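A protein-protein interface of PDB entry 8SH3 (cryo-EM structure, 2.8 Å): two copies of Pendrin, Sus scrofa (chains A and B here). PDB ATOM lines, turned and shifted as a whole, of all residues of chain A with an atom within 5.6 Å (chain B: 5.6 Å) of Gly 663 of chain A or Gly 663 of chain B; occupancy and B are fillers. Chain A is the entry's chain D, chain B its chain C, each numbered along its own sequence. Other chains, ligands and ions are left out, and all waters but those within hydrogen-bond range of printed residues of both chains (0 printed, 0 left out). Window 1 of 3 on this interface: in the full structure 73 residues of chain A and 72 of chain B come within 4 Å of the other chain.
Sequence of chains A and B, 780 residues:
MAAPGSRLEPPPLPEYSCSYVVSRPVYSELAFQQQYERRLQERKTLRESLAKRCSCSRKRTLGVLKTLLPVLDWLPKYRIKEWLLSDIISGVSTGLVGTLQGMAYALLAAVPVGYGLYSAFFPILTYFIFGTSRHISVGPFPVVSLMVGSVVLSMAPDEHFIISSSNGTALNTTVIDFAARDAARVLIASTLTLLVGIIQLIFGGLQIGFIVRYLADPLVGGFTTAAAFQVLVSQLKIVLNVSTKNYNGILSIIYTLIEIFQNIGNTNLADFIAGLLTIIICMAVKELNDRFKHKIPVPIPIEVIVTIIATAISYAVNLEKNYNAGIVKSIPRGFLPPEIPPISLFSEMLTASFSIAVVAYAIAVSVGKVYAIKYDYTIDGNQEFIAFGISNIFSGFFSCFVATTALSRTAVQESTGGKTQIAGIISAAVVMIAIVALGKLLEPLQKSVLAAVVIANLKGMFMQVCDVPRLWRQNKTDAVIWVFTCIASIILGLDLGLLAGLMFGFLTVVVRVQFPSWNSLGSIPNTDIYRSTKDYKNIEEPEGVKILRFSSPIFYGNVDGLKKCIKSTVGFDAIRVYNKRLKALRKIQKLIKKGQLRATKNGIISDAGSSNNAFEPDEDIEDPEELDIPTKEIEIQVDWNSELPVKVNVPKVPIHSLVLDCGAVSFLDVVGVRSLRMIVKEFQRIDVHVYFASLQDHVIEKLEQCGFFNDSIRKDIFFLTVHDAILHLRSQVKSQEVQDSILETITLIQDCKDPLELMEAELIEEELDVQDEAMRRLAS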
ATOM      1  N   ARG A 549     -15.532  -7.811  26.019  1.00  0.00           N
ATOM      2  CA  ARG A 549     -14.697  -7.052  26.942  1.00  0.00           C
ATOM      3  C   ARG A 549     -14.412  -7.942  28.144  1.00  0.00           C
ATOM      4  O   ARG A 549     -15.327  -8.284  28.901  1.00  0.00           O
ATOM      5  CB  ARG A 549     -15.383  -5.756  27.363  1.00  0.00           C
ATOM      6  CG  ARG A 549     -14.724  -5.038  28.530  1.00  0.00           C
ATOM      7  CD  ARG A 549     -13.298  -4.630  28.206  1.00  0.00           C
ATOM      8  NE  ARG A 549     -12.712  -3.804  29.256  1.00  0.00           N
ATOM      9  CZ  ARG A 549     -12.533  -2.493  29.166  1.00  0.00           C
ATOM     10  NH1 ARG A 549     -12.875  -1.821  28.081  1.00  0.00           N
ATOM     11  NH2 ARG A 549     -11.992  -1.842  30.192  1.00  0.00           N
ATOM     12  N   ASP A 661     -12.059  -6.718  23.236  1.00  0.00           N
ATOM     13  CA  ASP A 661     -11.772  -5.421  23.845  1.00  0.00           C
ATOM     14  C   ASP A 661     -10.828  -5.666  25.014  1.00  0.00           C
ATOM     15  O   ASP A 661     -11.250  -6.084  26.094  1.00  0.00           O
ATOM     16  CB  ASP A 661     -13.058  -4.736  24.291  1.00  0.00           C
ATOM     17  CG  ASP A 661     -12.826  -3.329  24.821  1.00  0.00           C
ATOM     18  OD1 ASP A 661     -11.657  -2.916  24.971  1.00  0.00           O
ATOM     19  OD2 ASP A 661     -13.824  -2.629  25.089  1.00  0.00           O
ATOM     20  N   CYS A 662      -9.542  -5.406  24.799  1.00  0.00           N
ATOM     21  CA  CYS A 662      -8.504  -5.673  25.790  1.00  0.00           C
ATOM     22  C   CYS A 662      -8.011  -4.397  26.458  1.00  0.00           C
ATOM     23  O   CYS A 662      -6.825  -4.270  26.774  1.00  0.00           O
ATOM     24  CB  CYS A 662      -7.346  -6.425  25.144  1.00  0.00           C
ATOM     25  SG  CYS A 662      -7.831  -7.876  24.188  1.00  0.00           S
ATOM     26  N   GLY A 663      -8.906  -3.434  26.682  1.00  0.00           N
ATOM     27  CA  GLY A 663      -8.509  -2.201  27.338  1.00  0.00           C
ATOM     28  C   GLY A 663      -8.073  -2.395  28.774  1.00  0.00           C
ATOM     29  O   GLY A 663      -7.175  -1.695  29.251  1.00  0.00           O
ATOM     30  N   ALA A 664      -8.695  -3.335  29.482  1.00  0.00           N
ATOM     31  CA  ALA A 664      -8.399  -3.575  30.886  1.00  0.00           C
ATOM     32  C   ALA A 664      -7.388  -4.690  31.105  1.00  0.00           C
ATOM     33  O   ALA A 664      -7.111  -5.037  32.257  1.00  0.00           O
ATOM     34  CB  ALA A 664      -9.685  -3.890  31.651  1.00  0.00           C
ATOM     35  N   VAL A 665      -6.832  -5.262  30.040  1.00  0.00           N
ATOM     36  CA  VAL A 665      -5.789  -6.271  30.176  1.00  0.00           C
ATOM     37  C   VAL A 665      -4.509  -5.574  30.611  1.00  0.00           C
ATOM     38  O   VAL A 665      -3.844  -4.911  29.807  1.00  0.00           O
ATOM     39  CB  VAL A 665      -5.586  -7.058  28.867  1.00  0.00           C
ATOM     40  CG1 VAL A 665      -4.405  -8.005  28.994  1.00  0.00           C
ATOM     41  CG2 VAL A 665      -6.850  -7.825  28.514  1.00  0.00           C
ATOM     42  N   ALA A 693      -8.309  -5.310  20.388  1.00  0.00           N
ATOM     43  CA  ALA A 693      -8.458  -3.865  20.402  1.00  0.00           C
ATOM     44  C   ALA A 693      -8.158  -3.321  21.790  1.00  0.00           C
ATOM     45  O   ALA A 693      -8.359  -4.002  22.800  1.00  0.00           O
ATOM     46  CB  ALA A 693      -9.862  -3.447  19.966  1.00  0.00           C
ATOM     47  N   SER A 694      -7.656  -2.087  21.821  1.00  0.00           N
ATOM     48  CA  SER A 694      -7.356  -1.347  23.046  1.00  0.00           C
ATOM     49  C   SER A 694      -6.232  -1.980  23.859  1.00  0.00           C
ATOM     50  O   SER A 694      -6.138  -1.751  25.069  1.00  0.00           O
ATOM     51  CB  SER A 694      -8.607  -1.176  23.914  1.00  0.00           C
ATOM     52  OG  SER A 694      -9.576  -0.370  23.266  1.00  0.00           O
ATOM     53  N   LEU A 695      -5.368  -2.771  23.227  1.00  0.00           N
ATOM     54  CA  LEU A 695      -4.198  -3.293  23.919  1.00  0.00           C
ATOM     55  C   LEU A 695      -3.158  -2.201  24.123  1.00  0.00           C
ATOM     56  O   LEU A 695      -2.936  -1.357  23.252  1.00  0.00           O
ATOM     57  CB  LEU A 695      -3.585  -4.456  23.144  1.00  0.00           C
ATOM     58  CG  LEU A 695      -4.194  -5.825  23.425  1.00  0.00           C
ATOM     59  CD1 LEU A 695      -3.663  -6.847  22.455  1.00  0.00           C
ATOM     60  CD2 LEU A 695      -3.866  -6.234  24.843  1.00  0.00           C
ATOM     61  N   GLN A 696      -2.513  -2.230  25.285  1.00  0.00           N
ATOM     62  CA  GLN A 696      -1.505  -1.240  25.618  1.00  0.00           C
ATOM     63  C   GLN A 696      -0.179  -1.567  24.937  1.00  0.00           C
ATOM     64  O   GLN A 696       0.029  -2.663  24.411  1.00  0.00           O
ATOM     65  CB  GLN A 696      -1.313  -1.159  27.130  1.00  0.00           C
ATOM     66  CG  GLN A 696      -2.454  -0.477  27.864  1.00  0.00           C
ATOM     67  CD  GLN A 696      -2.788   0.879  27.280  1.00  0.00           C
ATOM     68  OE1 GLN A 696      -3.775   1.032  26.560  1.00  0.00           O
ATOM     69  NE2 GLN A 696      -1.962   1.872  27.584  1.00  0.00           N
ATOM     70  N   ARG B 549      -2.409   7.493  32.904  1.00  0.00           N
ATOM     71  CA  ARG B 549      -2.939   6.150  32.703  1.00  0.00           C
ATOM     72  C   ARG B 549      -2.289   5.238  33.735  1.00  0.00           C
ATOM     73  O   ARG B 549      -1.077   5.005  33.689  1.00  0.00           O
ATOM     74  CB  ARG B 549      -2.669   5.661  31.282  1.00  0.00           C
ATOM     75  CG  ARG B 549      -2.926   4.178  31.062  1.00  0.00           C
ATOM     76  CD  ARG B 549      -4.375   3.812  31.321  1.00  0.00           C
ATOM     77  NE  ARG B 549      -4.668   2.429  30.966  1.00  0.00           N
ATOM     78  CZ  ARG B 549      -5.339   2.057  29.885  1.00  0.00           C
ATOM     79  NH1 ARG B 549      -5.817   2.945  29.030  1.00  0.00           N
ATOM     80  NH2 ARG B 549      -5.540   0.763  29.659  1.00  0.00           N
ATOM     81  N   ASP B 661      -6.920   8.366  33.268  1.00  0.00           N
ATOM     82  CA  ASP B 661      -7.373   7.372  32.298  1.00  0.00           C
ATOM     83  C   ASP B 661      -7.495   6.044  33.032  1.00  0.00           C
ATOM     84  O   ASP B 661      -6.499   5.361  33.282  1.00  0.00           O
ATOM     85  CB  ASP B 661      -6.409   7.283  31.122  1.00  0.00           C
ATOM     86  CG  ASP B 661      -6.759   6.164  30.152  1.00  0.00           C
ATOM     87  OD1 ASP B 661      -7.891   5.639  30.213  1.00  0.00           O
ATOM     88  OD2 ASP B 661      -5.906   5.825  29.308  1.00  0.00           O
ATOM     89  N   CYS B 662      -8.724   5.677  33.386  1.00  0.00           N
ATOM     90  CA  CYS B 662      -8.996   4.489  34.192  1.00  0.00           C
ATOM     91  C   CYS B 662      -9.560   3.350  33.355  1.00  0.00           C
ATOM     92  O   CYS B 662     -10.420   2.595  33.817  1.00  0.00           O
ATOM     93  CB  CYS B 662      -9.943   4.840  35.333  1.00  0.00           C
ATOM     94  SG  CYS B 662      -9.449   6.274  36.309  1.00  0.00           S
ATOM     95  N   GLY B 663      -9.092   3.206  32.114  1.00  0.00           N
ATOM     96  CA  GLY B 663      -9.567   2.124  31.272  1.00  0.00           C
ATOM     97  C   GLY B 663      -9.192   0.750  31.784  1.00  0.00           C
ATOM     98  O   GLY B 663      -9.957  -0.205  31.623  1.00  0.00           O
ATOM     99  N   ALA B 664      -8.018   0.624  32.397  1.00  0.00           N
ATOM    100  CA  ALA B 664      -7.525  -0.655  32.882  1.00  0.00           C
ATOM    101  C   ALA B 664      -7.832  -0.900  34.353  1.00  0.00           C
ATOM    102  O   ALA B 664      -7.400  -1.919  34.897  1.00  0.00           O
ATOM    103  CB  ALA B 664      -6.019  -0.766  32.647  1.00  0.00           C
ATOM    104  N   VAL B 665      -8.558   0.003  35.009  1.00  0.00           N
ATOM    105  CA  VAL B 665      -8.966  -0.213  36.393  1.00  0.00           C
ATOM    106  C   VAL B 665     -10.055  -1.276  36.403  1.00  0.00           C
ATOM    107  O   VAL B 665     -11.207  -1.007  36.044  1.00  0.00           O
ATOM    108  CB  VAL B 665      -9.444   1.093  37.052  1.00  0.00           C
ATOM    109  CG1 VAL B 665      -9.992   0.817  38.442  1.00  0.00           C
ATOM    110  CG2 VAL B 665      -8.304   2.096  37.119  1.00  0.00           C
ATOM    111  N   ALA B 693     -11.758   9.086  33.470  1.00  0.00           N
ATOM    112  CA  ALA B 693     -12.163   8.718  32.124  1.00  0.00           C
ATOM    113  C   ALA B 693     -11.976   7.224  31.910  1.00  0.00           C
ATOM    114  O   ALA B 693     -11.109   6.595  32.524  1.00  0.00           O
ATOM    115  CB  ALA B 693     -11.377   9.501  31.074  1.00  0.00           C
ATOM    116  N   SER B 694     -12.817   6.665  31.040  1.00  0.00           N
ATOM    117  CA  SER B 694     -12.776   5.260  30.638  1.00  0.00           C
ATOM    118  C   SER B 694     -13.082   4.306  31.788  1.00  0.00           C
ATOM    119  O   SER B 694     -12.683   3.139  31.750  1.00  0.00           O
ATOM    120  CB  SER B 694     -11.430   4.902  29.999  1.00  0.00           C
ATOM    121  OG  SER B 694     -11.237   5.602  28.782  1.00  0.00           O
ATOM    122  N   LEU B 695     -13.791   4.770  32.814  1.00  0.00           N
ATOM    123  CA  LEU B 695     -14.228   3.876  33.877  1.00  0.00           C
ATOM    124  C   LEU B 695     -15.388   3.008  33.412  1.00  0.00           C
ATOM    125  O   LEU B 695     -16.282   3.464  32.694  1.00  0.00           O
ATOM    126  CB  LEU B 695     -14.635   4.666  35.117  1.00  0.00           C
ATOM    127  CG  LEU B 695     -13.501   5.019  36.072  1.00  0.00           C
ATOM    128  CD1 LEU B 695     -13.984   5.968  37.138  1.00  0.00           C
ATOM    129  CD2 LEU B 695     -12.974   3.752  36.706  1.00  0.00           C
ATOM    130  N   GLN B 696     -15.372   1.748  33.836  1.00  0.00           N
ATOM    131  CA  GLN B 696     -16.414   0.808  33.467  1.00  0.00           C
ATOM    132  C   GLN B 696     -17.662   1.023  34.318  1.00  0.00           C
ATOM    133  O   GLN B 696     -17.638   1.699  35.349  1.00  0.00           O
ATOM    134  CB  GLN B 696     -15.917  -0.628  33.616  1.00  0.00           C
ATOM    135  CG  GLN B 696     -14.921  -1.054  32.552  1.00  0.00           C
ATOM    136  CD  GLN B 696     -15.427  -0.799  31.149  1.00  0.00           C
ATOM    137  OE1 GLN B 696     -15.012   0.156  30.490  1.00  0.00           O
ATOM    138  NE2 GLN B 696     -16.334  -1.650  30.683  1.00  0.00           N
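Printed residues of chain B within 4 Å of Arg 549 of chain A: Gly 663 (3.0 Å) and Gln 696 (3.6 Å).
Gly 663 of chain A touches just these residues of chain B: Arg 549 (3.0 Å), Gly 663 (3.9 Å) and Ala 664 (3.7 Å).
Printed residues of chain B within 4 Å of Ala 664 of chain A: Gly 663 (3.7 Å) and Ala 664 (3.6 Å).
Of the printed residues of chain B, Gln 696 of chain A touches Arg 549.
Of chain A, only Arg 549 (3.0 Å), Gly 663 (3.9 Å) and Ala 664 (3.7 Å) come within 4 Å of Gly 663 of chain B.
Of the printed residues of chain A, Ala 664 of chain B touches Gly 663 and Ala 664.
Val 665 of chain B touches none of the printed residues of chain A.
Ala 693 of chain B touches none of the printed residues of chain A.
Of the printed residues of chain A, Gln 696 of chain B touches Arg 549 (3.6 Å).
The nearest printed residue of chain A that does not touch Gly 663 of chain B is Val 665 of chain A (6.2 Å).
The nearest printed residue of chain A that does not touch Arg 549 of chain B is Ala 664 of chain A (5.2 Å).
O of Gly 663 of chain A lies within hydrogen-bond range of NH2 of Arg 549 of chain B, 3.0 Å away.
NH2 of Arg 549 of chain A sits at hydrogen-bond distance from O of Gly 663 of chain B (3.0 Å).
Among the printed residues, merely in contact across the chains: Arg 549 of chain A with Gln 696 of chain B (3.6 Å), Gly 663 of chain A with Gly 663 of chain B (3.9 Å), Gly 663 of chain A with Ala 664 of chain B (3.7 Å), Ala 664 of chain A with Gly 663 of chain B (3.7 Å), Ala 664 of chain A with Ala 664 of chain B (3.6 Å) and Gln 696 of chain A with Arg 549 of chain B (3.6 Å).
Arg 549 of chain A touches Gln 696 of chain B, and with the chains exchanged Gln 696 of chain A touches Arg 549 of chain B.
Gly 663 of chain B touches its own counterpart, Gly 663 of chain A.
Gly 663 of chain A touches Ala 664 of chain B, and with the chains exchanged Ala 664 of chain A touches Gly 663 of chain B.
Ala 664 of chain A touches its own counterpart, Ala 664 of chain B.
Positions printed for both chains: 549, 661, 662, 663, 664, 665, 693, 694, 695 and 696.
Of the 8 pairs that touch across the chains among the printed residues, 8 have their exchanged pair printed and touching as well.
NH1 of Arg 549 of chain B is in salt-bridge range of OD2 of Asp 661 of chain B (2.9 Å).
N of Gly 663 of chain B sits at hydrogen-bond distance from OD1 of Asp 661 of chain B (3.3 Å).
NH1 of Arg 549 of chain A lies within salt-bridge range of OD2 of Asp 661 of chain A (3.2 Å).
OD1 of Asp 661 of chain A sits at hydrogen-bond distance from N of Gly 663 of chain A, 3.3 Å away.
Printed residues of chain B that touch a printed residue of chain A: Arg 549, Gly 663, Ala 664 and Gln 696.
Among the printed residues, 8 pairs touch across the chains.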
